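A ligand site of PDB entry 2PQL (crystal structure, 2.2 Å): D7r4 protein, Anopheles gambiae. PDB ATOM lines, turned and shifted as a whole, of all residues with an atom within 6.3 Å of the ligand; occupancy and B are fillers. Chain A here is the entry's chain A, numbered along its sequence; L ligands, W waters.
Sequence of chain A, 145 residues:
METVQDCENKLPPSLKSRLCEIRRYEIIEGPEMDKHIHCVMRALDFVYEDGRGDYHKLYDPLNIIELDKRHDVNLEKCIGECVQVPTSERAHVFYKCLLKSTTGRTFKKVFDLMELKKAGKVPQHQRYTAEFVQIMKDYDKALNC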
ATOM      1  N   VAL A   4     -12.241  -6.437 -11.534  1.00  0.00           N
ATOM      2  CA  VAL A   4     -12.707  -7.149 -10.338  1.00  0.00           C
ATOM      3  C   VAL A   4     -13.506  -6.238  -9.400  1.00  0.00           C
ATOM      4  O   VAL A   4     -14.540  -6.653  -8.872  1.00  0.00           O
ATOM      5  CB  VAL A   4     -11.544  -7.766  -9.552  1.00  0.00           C
ATOM      6  CG1 VAL A   4     -12.042  -8.375  -8.256  1.00  0.00           C
ATOM      7  CG2 VAL A   4     -10.827  -8.811 -10.410  1.00  0.00           C
ATOM      8  N   GLU A   8     -17.261  -6.656  -8.045  1.00  0.00           N
ATOM      9  CA  GLU A   8     -17.665  -6.479  -6.650  1.00  0.00           C
ATOM     10  C   GLU A   8     -18.731  -5.387  -6.426  1.00  0.00           C
ATOM     11  O   GLU A   8     -19.669  -5.578  -5.657  1.00  0.00           O
ATOM     12  CB  GLU A   8     -16.435  -6.279  -5.756  1.00  0.00           C
ATOM     13  CG  GLU A   8     -15.412  -7.398  -5.900  1.00  0.00           C
ATOM     14  CD  GLU A   8     -14.282  -7.290  -4.906  1.00  0.00           C
ATOM     15  OE1 GLU A   8     -13.900  -6.147  -4.565  1.00  0.00           O
ATOM     16  OE2 GLU A   8     -13.763  -8.346  -4.477  1.00  0.00           O
ATOM     17  N   ILE A  22     -15.359 -14.527   0.180  1.00  0.00           N
ATOM     18  CA  ILE A  22     -15.017 -14.608  -1.236  1.00  0.00           C
ATOM     19  C   ILE A  22     -13.524 -14.312  -1.498  1.00  0.00           C
ATOM     20  O   ILE A  22     -12.825 -15.063  -2.198  1.00  0.00           O
ATOM     21  CB  ILE A  22     -15.892 -13.664  -2.069  1.00  0.00           C
ATOM     22  CG1 ILE A  22     -17.374 -13.951  -1.816  1.00  0.00           C
ATOM     23  CG2 ILE A  22     -15.574 -13.813  -3.555  1.00  0.00           C
ATOM     24  CD1 ILE A  22     -18.329 -12.990  -2.531  1.00  0.00           C
ATOM     25  N   ARG A  23     -13.030 -13.228  -0.925  1.00  0.00           N
ATOM     26  CA  ARG A  23     -11.699 -12.727  -1.250  1.00  0.00           C
ATOM     27  C   ARG A  23     -10.601 -13.530  -0.534  1.00  0.00           C
ATOM     28  O   ARG A  23      -9.406 -13.309  -0.760  1.00  0.00           O
ATOM     29  CB  ARG A  23     -11.598 -11.220  -0.943  1.00  0.00           C
ATOM     30  CG  ARG A  23     -12.383 -10.313  -1.915  1.00  0.00           C
ATOM     31  CD  ARG A  23     -12.069  -8.794  -1.705  1.00  0.00           C
ATOM     32  NE  ARG A  23     -10.659  -8.530  -1.968  1.00  0.00           N
ATOM     33  CZ  ARG A  23     -10.142  -8.294  -3.173  1.00  0.00           C
ATOM     34  NH1 ARG A  23     -10.928  -8.251  -4.243  1.00  0.00           N
ATOM     35  NH2 ARG A  23      -8.849  -8.091  -3.327  1.00  0.00           N
ATOM     36  N   ARG A  24     -11.019 -14.447   0.333  1.00  0.00           N
ATOM     37  CA  ARG A  24     -10.114 -15.404   0.987  1.00  0.00           C
ATOM     38  C   ARG A  24     -10.020 -16.688   0.161  1.00  0.00           C
ATOM     39  O   ARG A  24      -9.381 -17.633   0.582  1.00  0.00           O
ATOM     40  CB  ARG A  24     -10.656 -15.798   2.381  1.00  0.00           C
ATOM     41  CG  ARG A  24     -10.500 -14.736   3.441  1.00  0.00           C
ATOM     42  CD  ARG A  24     -10.546 -15.312   4.862  1.00  0.00           C
ATOM     43  NE  ARG A  24     -11.792 -16.000   5.198  1.00  0.00           N
ATOM     44  CZ  ARG A  24     -12.863 -15.408   5.743  1.00  0.00           C
ATOM     45  NH1 ARG A  24     -12.848 -14.105   5.980  1.00  0.00           N
ATOM     46  NH2 ARG A  24     -13.949 -16.120   6.022  1.00  0.00           N
ATOM     47  N   TYR A  25     -10.698 -16.694  -0.997  1.00  0.00           N
ATOM     48  CA  TYR A  25     -10.816 -17.879  -1.855  1.00  0.00           C
ATOM     49  C   TYR A  25     -11.678 -18.981  -1.263  1.00  0.00           C
ATOM     50  O   TYR A  25     -11.611 -20.161  -1.659  1.00  0.00           O
ATOM     51  CB  TYR A  25      -9.432 -18.427  -2.227  1.00  0.00           C
ATOM     52  CG  TYR A  25      -8.590 -17.485  -3.069  1.00  0.00           C
ATOM     53  CD1 TYR A  25      -8.711 -17.457  -4.451  1.00  0.00           C
ATOM     54  CD2 TYR A  25      -7.674 -16.627  -2.470  1.00  0.00           C
ATOM     55  CE1 TYR A  25      -7.946 -16.578  -5.234  1.00  0.00           C
ATOM     56  CE2 TYR A  25      -6.869 -15.762  -3.253  1.00  0.00           C
ATOM     57  CZ  TYR A  25      -7.031 -15.740  -4.615  1.00  0.00           C
ATOM     58  OH  TYR A  25      -6.268 -14.892  -5.388  1.00  0.00           O
ATOM     59  N   GLU A  26     -12.523 -18.618  -0.304  1.00  0.00           N
ATOM     60  CA  GLU A  26     -13.434 -19.594   0.247  1.00  0.00           C
ATOM     61  C   GLU A  26     -14.542 -19.915  -0.746  1.00  0.00           C
ATOM     62  O   GLU A  26     -14.972 -19.048  -1.513  1.00  0.00           O
ATOM     63  CB  GLU A  26     -13.944 -19.128   1.610  1.00  0.00           C
ATOM     64  CG  GLU A  26     -12.866 -19.276   2.683  1.00  0.00           C
ATOM     65  CD  GLU A  26     -13.170 -18.517   3.958  1.00  0.00           C
ATOM     66  OE1 GLU A  26     -14.350 -18.187   4.192  1.00  0.00           O
ATOM     67  OE2 GLU A  26     -12.224 -18.253   4.729  1.00  0.00           O
ATOM     68  N   MET A  33     -23.013 -16.671  -7.129  1.00  0.00           N
ATOM     69  CA  MET A  33     -21.563 -16.852  -7.111  1.00  0.00           C
ATOM     70  C   MET A  33     -21.040 -17.279  -8.473  1.00  0.00           C
ATOM     71  O   MET A  33     -19.929 -16.891  -8.871  1.00  0.00           O
ATOM     72  CB  MET A  33     -21.170 -17.867  -6.033  1.00  0.00           C
ATOM     73  CG  MET A  33     -20.896 -17.265  -4.661  1.00  0.00           C
ATOM     74  SD  MET A  33     -19.568 -16.021  -4.658  1.00  0.00           S
ATOM     75  CE  MET A  33     -18.095 -17.037  -4.807  1.00  0.00           C
ATOM     76  N   HIS A  36     -20.683 -14.001 -10.408  1.00  0.00           N
ATOM     77  CA  HIS A  36     -19.561 -13.220  -9.876  1.00  0.00           C
ATOM     78  C   HIS A  36     -18.214 -13.755 -10.388  1.00  0.00           C
ATOM     79  O   HIS A  36     -17.413 -13.020 -10.980  1.00  0.00           O
ATOM     80  CB  HIS A  36     -19.578 -13.196  -8.336  1.00  0.00           C
ATOM     81  CG  HIS A  36     -18.548 -12.308  -7.726  1.00  0.00           C
ATOM     82  ND1 HIS A  36     -18.413 -10.975  -8.048  1.00  0.00           N
ATOM     83  CD2 HIS A  36     -17.597 -12.556  -6.783  1.00  0.00           C
ATOM     84  CE1 HIS A  36     -17.434 -10.443  -7.337  1.00  0.00           C
ATOM     85  NE2 HIS A  36     -16.920 -11.378  -6.568  1.00  0.00           N
ATOM     86  N   ILE A  37     -17.972 -15.039 -10.182  1.00  0.00           N
ATOM     87  CA  ILE A  37     -16.705 -15.667 -10.554  1.00  0.00           C
ATOM     88  C   ILE A  37     -16.466 -15.679 -12.061  1.00  0.00           C
ATOM     89  O   ILE A  37     -15.316 -15.676 -12.517  1.00  0.00           O
ATOM     90  CB  ILE A  37     -16.590 -17.091  -9.989  1.00  0.00           C
ATOM     91  CG1 ILE A  37     -16.686 -17.060  -8.470  1.00  0.00           C
ATOM     92  CG2 ILE A  37     -15.294 -17.751 -10.451  1.00  0.00           C
ATOM     93  CD1 ILE A  37     -15.821 -15.977  -7.842  1.00  0.00           C
ATOM     94  N   VAL A  40     -15.324 -12.053 -12.647  1.00  0.00           N
ATOM     95  CA  VAL A  40     -13.945 -11.816 -12.231  1.00  0.00           C
ATOM     96  C   VAL A  40     -12.894 -12.577 -13.026  1.00  0.00           C
ATOM     97  O   VAL A  40     -11.860 -12.021 -13.375  1.00  0.00           O
ATOM     98  CB  VAL A  40     -13.702 -11.924 -10.697  1.00  0.00           C
ATOM     99  CG1 VAL A  40     -14.899 -11.471  -9.903  1.00  0.00           C
ATOM    100  CG2 VAL A  40     -13.200 -13.299 -10.278  1.00  0.00           C
ATOM    101  N   TYR A  95     -12.490 -22.452 -11.565  1.00  0.00           N
ATOM    102  CA  TYR A  95     -11.884 -21.748 -10.429  1.00  0.00           C
ATOM    103  C   TYR A  95     -11.856 -22.681  -9.226  1.00  0.00           C
ATOM    104  O   TYR A  95     -10.806 -22.868  -8.583  1.00  0.00           O
ATOM    105  CB  TYR A  95     -12.758 -20.511 -10.153  1.00  0.00           C
ATOM    106  CG  TYR A  95     -12.581 -19.751  -8.843  1.00  0.00           C
ATOM    107  CD1 TYR A  95     -11.635 -18.735  -8.724  1.00  0.00           C
ATOM    108  CD2 TYR A  95     -13.409 -20.011  -7.762  1.00  0.00           C
ATOM    109  CE1 TYR A  95     -11.509 -18.011  -7.534  1.00  0.00           C
ATOM    110  CE2 TYR A  95     -13.294 -19.306  -6.582  1.00  0.00           C
ATOM    111  CZ  TYR A  95     -12.340 -18.312  -6.473  1.00  0.00           C
ATOM    112  OH  TYR A  95     -12.237 -17.626  -5.294  1.00  0.00           O
ATOM    113  N   LEU A  99      -8.463 -24.436  -7.369  1.00  0.00           N
ATOM    114  CA  LEU A  99      -8.196 -24.145  -5.967  1.00  0.00           C
ATOM    115  C   LEU A  99      -8.060 -25.409  -5.142  1.00  0.00           C
ATOM    116  O   LEU A  99      -7.312 -25.430  -4.162  1.00  0.00           O
ATOM    117  CB  LEU A  99      -9.280 -23.221  -5.383  1.00  0.00           C
ATOM    118  CG  LEU A  99      -9.161 -21.736  -5.785  1.00  0.00           C
ATOM    119  CD1 LEU A  99     -10.385 -20.941  -5.372  1.00  0.00           C
ATOM    120  CD2 LEU A  99      -7.894 -21.128  -5.171  1.00  0.00           C
ATOM    121  N   LYS A 108      -3.524 -18.855  -6.474  1.00  0.00           N
ATOM    122  CA  LYS A 108      -3.879 -17.691  -5.651  1.00  0.00           C
ATOM    123  C   LYS A 108      -2.869 -16.551  -5.772  1.00  0.00           C
ATOM    124  O   LYS A 108      -3.233 -15.376  -5.749  1.00  0.00           O
ATOM    125  CB  LYS A 108      -4.041 -18.096  -4.192  1.00  0.00           C
ATOM    126  CG  LYS A 108      -5.296 -18.904  -3.895  1.00  0.00           C
ATOM    127  CD  LYS A 108      -5.405 -19.264  -2.385  1.00  0.00           C
ATOM    128  CE  LYS A 108      -4.518 -20.491  -2.061  1.00  0.00           C
ATOM    129  NZ  LYS A 108      -4.596 -20.974  -0.631  1.00  0.00           N
ATOM    130  N   PHE A 111      -3.337 -15.103  -9.302  1.00  0.00           N
ATOM    131  CA  PHE A 111      -4.602 -14.375  -9.199  1.00  0.00           C
ATOM    132  C   PHE A 111      -4.448 -13.022  -8.471  1.00  0.00           C
ATOM    133  O   PHE A 111      -4.878 -11.993  -8.979  1.00  0.00           O
ATOM    134  CB  PHE A 111      -5.630 -15.282  -8.499  1.00  0.00           C
ATOM    135  CG  PHE A 111      -7.041 -14.753  -8.498  1.00  0.00           C
ATOM    136  CD1 PHE A 111      -7.375 -13.600  -7.805  1.00  0.00           C
ATOM    137  CD2 PHE A 111      -8.055 -15.462  -9.148  1.00  0.00           C
ATOM    138  CE1 PHE A 111      -8.691 -13.129  -7.782  1.00  0.00           C
ATOM    139  CE2 PHE A 111      -9.372 -15.001  -9.126  1.00  0.00           C
ATOM    140  CZ  PHE A 111      -9.685 -13.840  -8.443  1.00  0.00           C
ATOM    141  N   ASP A 112      -3.822 -13.032  -7.293  1.00  0.00           N
ATOM    142  CA  ASP A 112      -3.516 -11.782  -6.572  1.00  0.00           C
ATOM    143  C   ASP A 112      -2.710 -10.797  -7.435  1.00  0.00           C
ATOM    144  O   ASP A 112      -3.043  -9.615  -7.502  1.00  0.00           O
ATOM    145  CB  ASP A 112      -2.703 -12.078  -5.301  1.00  0.00           C
ATOM    146  CG  ASP A 112      -3.539 -12.669  -4.180  1.00  0.00           C
ATOM    147  OD1 ASP A 112      -4.758 -12.879  -4.385  1.00  0.00           O
ATOM    148  OD2 ASP A 112      -2.972 -12.925  -3.102  1.00  0.00           O
ATOM    149  N   GLU A 115      -4.722  -9.339 -10.234  1.00  0.00           N
ATOM    150  CA  GLU A 115      -5.745  -8.420  -9.769  1.00  0.00           C
ATOM    151  C   GLU A 115      -5.131  -7.046  -9.595  1.00  0.00           C
ATOM    152  O   GLU A 115      -5.674  -6.049 -10.094  1.00  0.00           O
ATOM    153  CB  GLU A 115      -6.353  -8.899  -8.445  1.00  0.00           C
ATOM    154  CG  GLU A 115      -7.619  -8.131  -8.063  1.00  0.00           C
ATOM    155  CD  GLU A 115      -8.003  -8.307  -6.597  1.00  0.00           C
ATOM    156  OE1 GLU A 115      -7.367  -9.122  -5.887  1.00  0.00           O
ATOM    157  OE2 GLU A 115      -8.945  -7.626  -6.150  1.00  0.00           O
ATOM    158  N   MET A 136      -0.964  -6.556  -0.854  1.00  0.00           N
ATOM    159  CA  MET A 136      -2.236  -7.253  -0.928  1.00  0.00           C
ATOM    160  C   MET A 136      -3.055  -7.133   0.371  1.00  0.00           C
ATOM    161  O   MET A 136      -4.267  -6.871   0.326  1.00  0.00           O
ATOM    162  CB  MET A 136      -2.030  -8.706  -1.372  1.00  0.00           C
ATOM    163  CG  MET A 136      -3.327  -9.501  -1.646  1.00  0.00           C
ATOM    164  SD  MET A 136      -4.160  -9.134  -3.227  1.00  0.00           S
ATOM    165  CE  MET A 136      -5.399  -8.006  -2.605  1.00  0.00           C
ATOM    166  N   ASP A 140      -6.699  -5.293   0.702  1.00  0.00           N
ATOM    167  CA  ASP A 140      -7.855  -5.949   1.309  1.00  0.00           C
ATOM    168  C   ASP A 140      -8.398  -5.179   2.501  1.00  0.00           C
ATOM    169  O   ASP A 140      -9.607  -5.088   2.696  1.00  0.00           O
ATOM    170  CB  ASP A 140      -7.519  -7.391   1.737  1.00  0.00           C
ATOM    171  CG  ASP A 140      -7.547  -8.384   0.570  1.00  0.00           C
ATOM    172  OD1 ASP A 140      -8.078  -8.050  -0.508  1.00  0.00           O
ATOM    173  OD2 ASP A 140      -7.020  -9.501   0.739  1.00  0.00           O
HETATM  174  N1  LIG L   1      -6.976 -11.128  -3.946  1.00  0.00           N
HETATM  175  C1  LIG L   1      -7.909 -12.225  -4.115  1.00  0.00           C
HETATM  176  C2  LIG L   1      -9.337 -11.674  -4.204  1.00  0.00           C
HETATM  177  C3  LIG L   1     -10.269 -12.802  -4.612  1.00  0.00           C
HETATM  178  C4  LIG L   1     -10.125 -14.178  -4.367  1.00  0.00           C
HETATM  179  N2  LIG L   1     -11.162 -14.895  -4.918  1.00  0.00           N
HETATM  180  C5  LIG L   1     -11.962 -13.987  -5.500  1.00  0.00           C
HETATM  181  C6  LIG L   1     -11.439 -12.745  -5.327  1.00  0.00           C
HETATM  182  C7  LIG L   1     -13.132 -14.282  -6.164  1.00  0.00           C
HETATM  183  C8  LIG L   1     -13.827 -13.171  -6.615  1.00  0.00           C
HETATM  184  C9  LIG L   1     -13.249 -11.894  -6.572  1.00  0.00           C
HETATM  185  C10 LIG L   1     -12.093 -11.638  -5.838  1.00  0.00           C
HETATM  186  O   HOH W   1      -7.326 -11.075  -1.331  1.00  0.00           O
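A nitrogen (N2) of the ligand is in hydrogen-bond range of the backbone carbonyl oxygen (O) of Ile 22. The side-chain carboxylate (OE1) of Glu 115 is in salt-bridge range of a nitrogen (N1) of the ligand, at 2.8 Å. The side-chain hydroxyl (OH) of Tyr 95 is in hydrogen-bond range of a nitrogen (N2) of the ligand (3.0 Å). SD of Met 136 is in hydrogen-bond range of N1 of the ligand, 3.5 Å away. A nitrogen (N1) of the ligand is in salt-bridge range of the side-chain carboxylate (OD1) of Asp 112 (2.9 Å).
Merely in contact with the ligand: Tyr 25 (3.4 Å), Phe 111 (3.6 Å), His 36 (3.6 Å), Ile 37 (3.6 Å), Arg 23 (3.6 Å), Val 40 (3.7 Å) and Glu 8 (3.9 Å). Hydrophobic or aromatic side chains within 4 Å of the ligand: Ile 22, Tyr 25, His 36, Ile 37, Val 40, Tyr 95, Phe 111 and Met 136. Of the 19 residues printed, 12 come within 4 Å of the ligand. Along chain A the residues within 4 Å of the ligand span positions 8 to 136. The nearest printed residue that does not touch the ligand is Val 4 (4.1 Å).
The side-chain carboxylate of Glu 115 is in salt-bridge range of the guanidinium group of Arg 23 (2.8 Å). The side-chain hydroxyl (OH) of Tyr 25 is in hydrogen-bond range of the backbone carbonyl oxygen (O) of Lys 108, at 3.1 Å. NH2 of Arg 23 lies within salt-bridge range of OD1 of Asp 140 (2.9 Å). OH of Tyr 25 lies within hydrogen-bond range of OD1 of Asp 112 (2.7 Å). The side-chain carboxylate (OE2) of Glu 8 is in salt-bridge range of the guanidinium group (NH1) of Arg 23, 2.8 Å away.
Water W1 lies within hydrogen-bond range of OD2 of Asp 140 (2.6 Å), N1 of the ligand (2.6 Å) and O of Arg 23 (3.1 Å).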
